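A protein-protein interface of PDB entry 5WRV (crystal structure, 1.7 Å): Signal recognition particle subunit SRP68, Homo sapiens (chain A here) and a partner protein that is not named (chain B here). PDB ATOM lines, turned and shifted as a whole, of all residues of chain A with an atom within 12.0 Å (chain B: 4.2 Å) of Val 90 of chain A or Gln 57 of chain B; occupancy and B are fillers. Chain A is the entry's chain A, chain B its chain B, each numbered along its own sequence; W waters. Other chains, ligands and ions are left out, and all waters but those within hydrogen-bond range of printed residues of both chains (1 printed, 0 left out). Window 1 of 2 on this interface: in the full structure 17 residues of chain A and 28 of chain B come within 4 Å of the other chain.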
ATOM      1  N   PHE A  83       1.590 -29.975  16.985  1.00  0.00           N
ATOM      2  CA  PHE A  83       1.815 -29.267  15.719  1.00  0.00           C
ATOM      3  C   PHE A  83       2.745 -28.071  15.866  1.00  0.00           C
ATOM      4  O   PHE A  83       2.596 -27.276  16.799  1.00  0.00           O
ATOM      5  CB  PHE A  83       0.484 -28.776  15.138  1.00  0.00           C
ATOM      6  CG  PHE A  83      -0.441 -29.882  14.727  1.00  0.00           C
ATOM      7  CD1 PHE A  83      -0.224 -30.588  13.546  1.00  0.00           C
ATOM      8  CD2 PHE A  83      -1.535 -30.216  15.518  1.00  0.00           C
ATOM      9  CE1 PHE A  83      -1.079 -31.612  13.165  1.00  0.00           C
ATOM     10  CE2 PHE A  83      -2.396 -31.240  15.139  1.00  0.00           C
ATOM     11  CZ  PHE A  83      -2.165 -31.938  13.963  1.00  0.00           C
ATOM     12  N   ASP A  84       3.689 -27.941  14.931  1.00  0.00           N
ATOM     13  CA  ASP A  84       4.503 -26.729  14.818  1.00  0.00           C
ATOM     14  C   ASP A  84       3.696 -25.664  14.078  1.00  0.00           C
ATOM     15  O   ASP A  84       3.865 -25.461  12.864  1.00  0.00           O
ATOM     16  CB  ASP A  84       5.831 -27.031  14.098  1.00  0.00           C
ATOM     17  CG  ASP A  84       6.707 -25.788  13.900  1.00  0.00           C
ATOM     18  OD1 ASP A  84       6.372 -24.688  14.397  1.00  0.00           O
ATOM     19  OD2 ASP A  84       7.757 -25.919  13.243  1.00  0.00           O
ATOM     20  N   LEU A  85       2.820 -24.981  14.807  1.00  0.00           N
ATOM     21  CA  LEU A  85       2.009 -23.905  14.220  1.00  0.00           C
ATOM     22  C   LEU A  85       2.815 -22.633  13.977  1.00  0.00           C
ATOM     23  O   LEU A  85       2.445 -21.813  13.136  1.00  0.00           O
ATOM     24  CB  LEU A  85       0.775 -23.603  15.083  1.00  0.00           C
ATOM     25  CG  LEU A  85      -0.195 -24.775  15.248  1.00  0.00           C
ATOM     26  CD1 LEU A  85      -1.328 -24.405  16.197  1.00  0.00           C
ATOM     27  CD2 LEU A  85      -0.731 -25.249  13.897  1.00  0.00           C
ATOM     28  N   ALA A  86       3.921 -22.466  14.703  1.00  0.00           N
ATOM     29  CA  ALA A  86       4.810 -21.322  14.470  1.00  0.00           C
ATOM     30  C   ALA A  86       5.290 -21.254  13.011  1.00  0.00           C
ATOM     31  O   ALA A  86       5.420 -20.161  12.444  1.00  0.00           O
ATOM     32  CB  ALA A  86       5.997 -21.351  15.433  1.00  0.00           C
ATOM     33  N   LEU A  87       5.535 -22.412  12.408  1.00  0.00           N
ATOM     34  CA  LEU A  87       5.981 -22.482  11.000  1.00  0.00           C
ATOM     35  C   LEU A  87       5.000 -21.791  10.053  1.00  0.00           C
ATOM     36  O   LEU A  87       5.415 -21.158   9.065  1.00  0.00           O
ATOM     37  CB  LEU A  87       6.202 -23.932  10.568  1.00  0.00           C
ATOM     38  CG  LEU A  87       6.678 -24.214   9.131  1.00  0.00           C
ATOM     39  CD1 LEU A  87       7.929 -23.415   8.782  1.00  0.00           C
ATOM     40  CD2 LEU A  87       6.940 -25.706   8.956  1.00  0.00           C
ATOM     41  N   ASN A  88       3.711 -21.896  10.368  1.00  0.00           N
ATOM     42  CA  ASN A  88       2.657 -21.248   9.571  1.00  0.00           C
ATOM     43  C   ASN A  88       2.725 -19.718   9.587  1.00  0.00           C
ATOM     44  O   ASN A  88       2.145 -19.072   8.722  1.00  0.00           O
ATOM     45  CB  ASN A  88       1.271 -21.688  10.050  1.00  0.00           C
ATOM     46  CG  ASN A  88       1.011 -23.163   9.830  1.00  0.00           C
ATOM     47  OD1 ASN A  88       1.408 -23.740   8.823  1.00  0.00           O
ATOM     48  ND2 ASN A  88       0.318 -23.776  10.773  1.00  0.00           N
ATOM     49  N   HIS A  89       3.413 -19.153  10.583  1.00  0.00           N
ATOM     50  CA  HIS A  89       3.561 -17.701  10.737  1.00  0.00           C
ATOM     51  C   HIS A  89       4.837 -17.149  10.133  1.00  0.00           C
ATOM     52  O   HIS A  89       5.092 -15.942  10.210  1.00  0.00           O
ATOM     53  CB  HIS A  89       3.491 -17.299  12.220  1.00  0.00           C
ATOM     54  CG  HIS A  89       2.279 -17.830  12.949  1.00  0.00           C
ATOM     55  ND1 HIS A  89       1.034 -17.744  12.448  1.00  0.00           N
ATOM     56  CD2 HIS A  89       2.161 -18.454  14.188  1.00  0.00           C
ATOM     57  CE1 HIS A  89       0.163 -18.293  13.315  1.00  0.00           C
ATOM     58  NE2 HIS A  89       0.857 -18.725  14.383  1.00  0.00           N
ATOM     59  N   VAL A  90       5.658 -18.019   9.548  1.00  0.00           N
ATOM     60  CA  VAL A  90       6.917 -17.609   8.920  1.00  0.00           C
ATOM     61  C   VAL A  90       6.571 -17.059   7.532  1.00  0.00           C
ATOM     62  O   VAL A  90       6.366 -17.825   6.581  1.00  0.00           O
ATOM     63  CB  VAL A  90       7.927 -18.784   8.825  1.00  0.00           C
ATOM     64  CG1 VAL A  90       9.191 -18.370   8.072  1.00  0.00           C
ATOM     65  CG2 VAL A  90       8.290 -19.300  10.222  1.00  0.00           C
ATOM     66  N   ALA A  91       6.479 -15.732   7.446  1.00  0.00           N
ATOM     67  CA  ALA A  91       5.939 -15.050   6.267  1.00  0.00           C
ATOM     68  C   ALA A  91       6.608 -13.698   6.059  1.00  0.00           C
ATOM     69  O   ALA A  91       7.063 -13.065   7.016  1.00  0.00           O
ATOM     70  CB  ALA A  91       4.430 -14.865   6.418  1.00  0.00           C
ATOM     71  N   PHE A  92       6.659 -13.256   4.803  1.00  0.00           N
ATOM     72  CA  PHE A  92       7.189 -11.932   4.487  1.00  0.00           C
ATOM     73  C   PHE A  92       6.425 -10.849   5.244  1.00  0.00           C
ATOM     74  O   PHE A  92       5.214 -10.972   5.464  1.00  0.00           O
ATOM     75  CB  PHE A  92       7.054 -11.623   2.982  1.00  0.00           C
ATOM     76  CG  PHE A  92       7.889 -12.489   2.078  1.00  0.00           C
ATOM     77  CD1 PHE A  92       8.927 -13.283   2.563  1.00  0.00           C
ATOM     78  CD2 PHE A  92       7.650 -12.474   0.694  1.00  0.00           C
ATOM     79  CE1 PHE A  92       9.685 -14.072   1.696  1.00  0.00           C
ATOM     80  CE2 PHE A  92       8.410 -13.251  -0.175  1.00  0.00           C
ATOM     81  CZ  PHE A  92       9.432 -14.050   0.324  1.00  0.00           C
ATOM     82  N   PRO A  93       7.129  -9.768   5.629  1.00  0.00           N
ATOM     83  CA  PRO A  93       6.481  -8.571   6.161  1.00  0.00           C
ATOM     84  C   PRO A  93       5.685  -7.880   5.040  1.00  0.00           C
ATOM     85  O   PRO A  93       5.857  -8.245   3.873  1.00  0.00           O
ATOM     86  CB  PRO A  93       7.670  -7.701   6.583  1.00  0.00           C
ATOM     87  CG  PRO A  93       8.771  -8.103   5.658  1.00  0.00           C
ATOM     88  CD  PRO A  93       8.586  -9.587   5.472  1.00  0.00           C
ATOM     89  N   PRO A  94       4.830  -6.893   5.375  1.00  0.00           N
ATOM     90  CA  PRO A  94       4.112  -6.157   4.321  1.00  0.00           C
ATOM     91  C   PRO A  94       5.067  -5.560   3.283  1.00  0.00           C
ATOM     92  O   PRO A  94       6.106  -5.007   3.648  1.00  0.00           O
ATOM     93  CB  PRO A  94       3.401  -5.047   5.096  1.00  0.00           C
ATOM     94  CG  PRO A  94       3.188  -5.633   6.458  1.00  0.00           C
ATOM     95  CD  PRO A  94       4.419  -6.452   6.724  1.00  0.00           C
ATOM     96  N   LEU A  95       4.725  -5.680   2.003  1.00  0.00           N
ATOM     97  CA  LEU A  95       5.647  -5.255   0.944  1.00  0.00           C
ATOM     98  C   LEU A  95       5.202  -4.029   0.139  1.00  0.00           C
ATOM     99  O   LEU A  95       5.914  -3.603  -0.777  1.00  0.00           O
ATOM    100  CB  LEU A  95       5.969  -6.419  -0.002  1.00  0.00           C
ATOM    101  CG  LEU A  95       6.734  -7.616   0.586  1.00  0.00           C
ATOM    102  CD1 LEU A  95       7.081  -8.602  -0.518  1.00  0.00           C
ATOM    103  CD2 LEU A  95       7.995  -7.209   1.344  1.00  0.00           C
ATOM    104  N   PHE B  27       9.542 -19.980  -2.629  1.00  0.00           N
ATOM    105  CA  PHE B  27      10.546 -19.281  -1.828  1.00  0.00           C
ATOM    106  C   PHE B  27      11.928 -19.383  -2.444  1.00  0.00           C
ATOM    107  O   PHE B  27      12.763 -18.493  -2.244  1.00  0.00           O
ATOM    108  CB  PHE B  27      10.500 -19.746  -0.363  1.00  0.00           C
ATOM    109  CG  PHE B  27       9.223 -19.367   0.313  1.00  0.00           C
ATOM    110  CD1 PHE B  27       9.010 -18.050   0.731  1.00  0.00           C
ATOM    111  CD2 PHE B  27       8.191 -20.299   0.461  1.00  0.00           C
ATOM    112  CE1 PHE B  27       7.808 -17.675   1.318  1.00  0.00           C
ATOM    113  CE2 PHE B  27       6.987 -19.925   1.051  1.00  0.00           C
ATOM    114  CZ  PHE B  27       6.799 -18.613   1.476  1.00  0.00           C
ATOM    115  N   VAL B  53      13.058 -15.398   5.804  1.00  0.00           N
ATOM    116  CA  VAL B  53      11.825 -16.178   5.586  1.00  0.00           C
ATOM    117  C   VAL B  53      12.011 -17.254   4.505  1.00  0.00           C
ATOM    118  O   VAL B  53      11.631 -18.412   4.707  1.00  0.00           O
ATOM    119  CB  VAL B  53      10.617 -15.264   5.281  1.00  0.00           C
ATOM    120  CG1 VAL B  53       9.401 -16.072   4.826  1.00  0.00           C
ATOM    121  CG2 VAL B  53      10.264 -14.440   6.510  1.00  0.00           C
ATOM    122  N   CYS B  54      12.604 -16.888   3.367  1.00  0.00           N
ATOM    123  CA  CYS B  54      12.831 -17.863   2.294  1.00  0.00           C
ATOM    124  C   CYS B  54      13.695 -19.026   2.780  1.00  0.00           C
ATOM    125  O   CYS B  54      13.407 -20.182   2.501  1.00  0.00           O
ATOM    126  CB  CYS B  54      13.525 -17.218   1.092  1.00  0.00           C
ATOM    127  SG  CYS B  54      12.523 -16.022   0.177  1.00  0.00           S
ATOM    128  N   LEU B  55      14.769 -18.700   3.494  1.00  0.00           N
ATOM    129  CA  LEU B  55      15.699 -19.716   3.972  1.00  0.00           C
ATOM    130  C   LEU B  55      14.998 -20.671   4.941  1.00  0.00           C
ATOM    131  O   LEU B  55      15.141 -21.896   4.822  1.00  0.00           O
ATOM    132  CB  LEU B  55      16.920 -19.046   4.613  1.00  0.00           C
ATOM    133  CG  LEU B  55      17.842 -18.372   3.582  1.00  0.00           C
ATOM    134  CD1 LEU B  55      18.811 -17.423   4.272  1.00  0.00           C
ATOM    135  CD2 LEU B  55      18.579 -19.419   2.747  1.00  0.00           C
ATOM    136  N   ILE B  56      14.211 -20.118   5.867  1.00  0.00           N
ATOM    137  CA  ILE B  56      13.464 -20.951   6.827  1.00  0.00           C
ATOM    138  C   ILE B  56      12.490 -21.863   6.071  1.00  0.00           C
ATOM    139  O   ILE B  56      12.407 -23.076   6.321  1.00  0.00           O
ATOM    140  CB  ILE B  56      12.704 -20.105   7.871  1.00  0.00           C
ATOM    141  CG1 ILE B  56      13.705 -19.381   8.794  1.00  0.00           C
ATOM    142  CG2 ILE B  56      11.779 -20.995   8.704  1.00  0.00           C
ATOM    143  CD1 ILE B  56      13.087 -18.307   9.671  1.00  0.00           C
ATOM    144  N   GLN B  57      11.777 -21.281   5.116  1.00  0.00           N
ATOM    145  CA  GLN B  57      10.810 -22.049   4.325  1.00  0.00           C
ATOM    146  C   GLN B  57      11.452 -23.202   3.558  1.00  0.00           C
ATOM    147  O   GLN B  57      10.812 -24.232   3.333  1.00  0.00           O
ATOM    148  CB  GLN B  57      10.062 -21.116   3.363  1.00  0.00           C
ATOM    149  CG  GLN B  57       9.028 -20.229   4.053  1.00  0.00           C
ATOM    150  CD  GLN B  57       7.785 -20.988   4.493  1.00  0.00           C
ATOM    151  OE1 GLN B  57       7.559 -22.125   4.086  1.00  0.00           O
ATOM    152  NE2 GLN B  57       6.976 -20.359   5.332  1.00  0.00           N
ATOM    153  N   ASN B  58      12.714 -23.029   3.161  1.00  0.00           N
ATOM    154  CA  ASN B  58      13.449 -24.086   2.457  1.00  0.00           C
ATOM    155  C   ASN B  58      14.316 -24.947   3.383  1.00  0.00           C
ATOM    156  O   ASN B  58      15.130 -25.739   2.913  1.00  0.00           O
ATOM    157  CB  ASN B  58      14.285 -23.495   1.306  1.00  0.00           C
ATOM    158  CG  ASN B  58      13.443 -23.145   0.090  1.00  0.00           C
ATOM    159  OD1 ASN B  58      12.254 -23.469   0.020  1.00  0.00           O
ATOM    160  ND2 ASN B  58      14.063 -22.480  -0.884  1.00  0.00           N
ATOM    161  N   GLY B  59      14.137 -24.778   4.694  1.00  0.00           N
ATOM    162  CA  GLY B  59      14.817 -25.613   5.691  1.00  0.00           C
ATOM    163  C   GLY B  59      16.275 -25.264   5.958  1.00  0.00           C
ATOM    164  O   GLY B  59      17.000 -26.062   6.545  1.00  0.00           O
ATOM    165  N   PHE B  82      11.421 -13.193  16.279  1.00  0.00           N
ATOM    166  CA  PHE B  82      10.631 -14.396  15.994  1.00  0.00           C
ATOM    167  C   PHE B  82      11.422 -15.370  15.125  1.00  0.00           C
ATOM    168  O   PHE B  82      11.538 -16.554  15.458  1.00  0.00           O
ATOM    169  CB  PHE B  82       9.285 -14.058  15.332  1.00  0.00           C
ATOM    170  CG  PHE B  82       8.579 -15.259  14.764  1.00  0.00           C
ATOM    171  CD1 PHE B  82       7.958 -16.185  15.603  1.00  0.00           C
ATOM    172  CD2 PHE B  82       8.549 -15.478  13.383  1.00  0.00           C
ATOM    173  CE1 PHE B  82       7.310 -17.300  15.081  1.00  0.00           C
ATOM    174  CE2 PHE B  82       7.901 -16.589  12.858  1.00  0.00           C
ATOM    175  CZ  PHE B  82       7.280 -17.501  13.703  1.00  0.00           C
HETATM  176  O   HOH W   1       4.631 -21.549   6.446  1.00  0.00           O
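The backbone carbonyl oxygen (O) of Val 90 of chain A sits at hydrogen-bond distance from the side-chain amide nitrogen (NE2) of Gln 57 of chain B (2.9 Å).
The backbone NH (N) of Ala 86 of chain A sits close to the side-chain carboxylate (OD1) of Asp 84 of chain A. The backbone carbonyl oxygen (O) of Phe 27 of chain B sits at hydrogen-bond distance from the side-chain sulfur (SG) of Cys 54 of chain B, at 3.5 Å.
Among the printed residues, merely in contact across the chains: Ala 86 of chain A with Phe 82 of chain B, Ala 91 of chain A with Val 53 of chain B, Phe 92 of chain A with Val 53 of chain B, Phe 92 of chain A with Cys 54 of chain B, Val 90 of chain A with Ile 56 of chain B, Val 90 of chain A with Phe 82 of chain B, His 89 of chain A with Phe 82 of chain B and Val 90 of chain A with Val 53 of chain B.
Val 90 of chain A touches four residues of chain B. Gln 57 of chain B touches one residue of chain A. No residue of chain A comes within 4 Å of Phe 27 of chain B. Val 53 of chain B touches three residues of chain A. No residue of chain A comes within 4 Å of Asn 58 of chain B. Printed residues of chain A within 4 Å of Phe 82 of chain B: Ala 86 (3.5 Å), His 89 (3.9 Å) and Val 90 (3.8 Å). Of the printed residues of chain B, Phe 92 of chain A touches Val 53 and Cys 54. Printed residues of chain B within 4 Å of His 89 of chain A: Phe 82 (3.9 Å). Printed residues of chain B within 4 Å of Ala 91 of chain A: Val 53. Leu 85 of chain A touches none of the printed residues of chain B.
Along chain B the printed residues that touch a printed residue of chain A span positions 53 to 82. Printed residues of chain A that touch a printed residue of chain B: Ala 86, His 89, Val 90, Ala 91 and Phe 92. Among the printed residues, 9 pairs touch across the chains. Among the printed residues, no Asp or Glu carboxylate lies within 4 Å of a Lys or Arg side-chain nitrogen of the other chain.
Water W1 lies within hydrogen-bond range of the backbone carbonyl oxygen (O) of Leu 87 of chain A (2.8 Å) and the side-chain amide nitrogen (NE2) of Gln 57 of chain B (2.9 Å).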
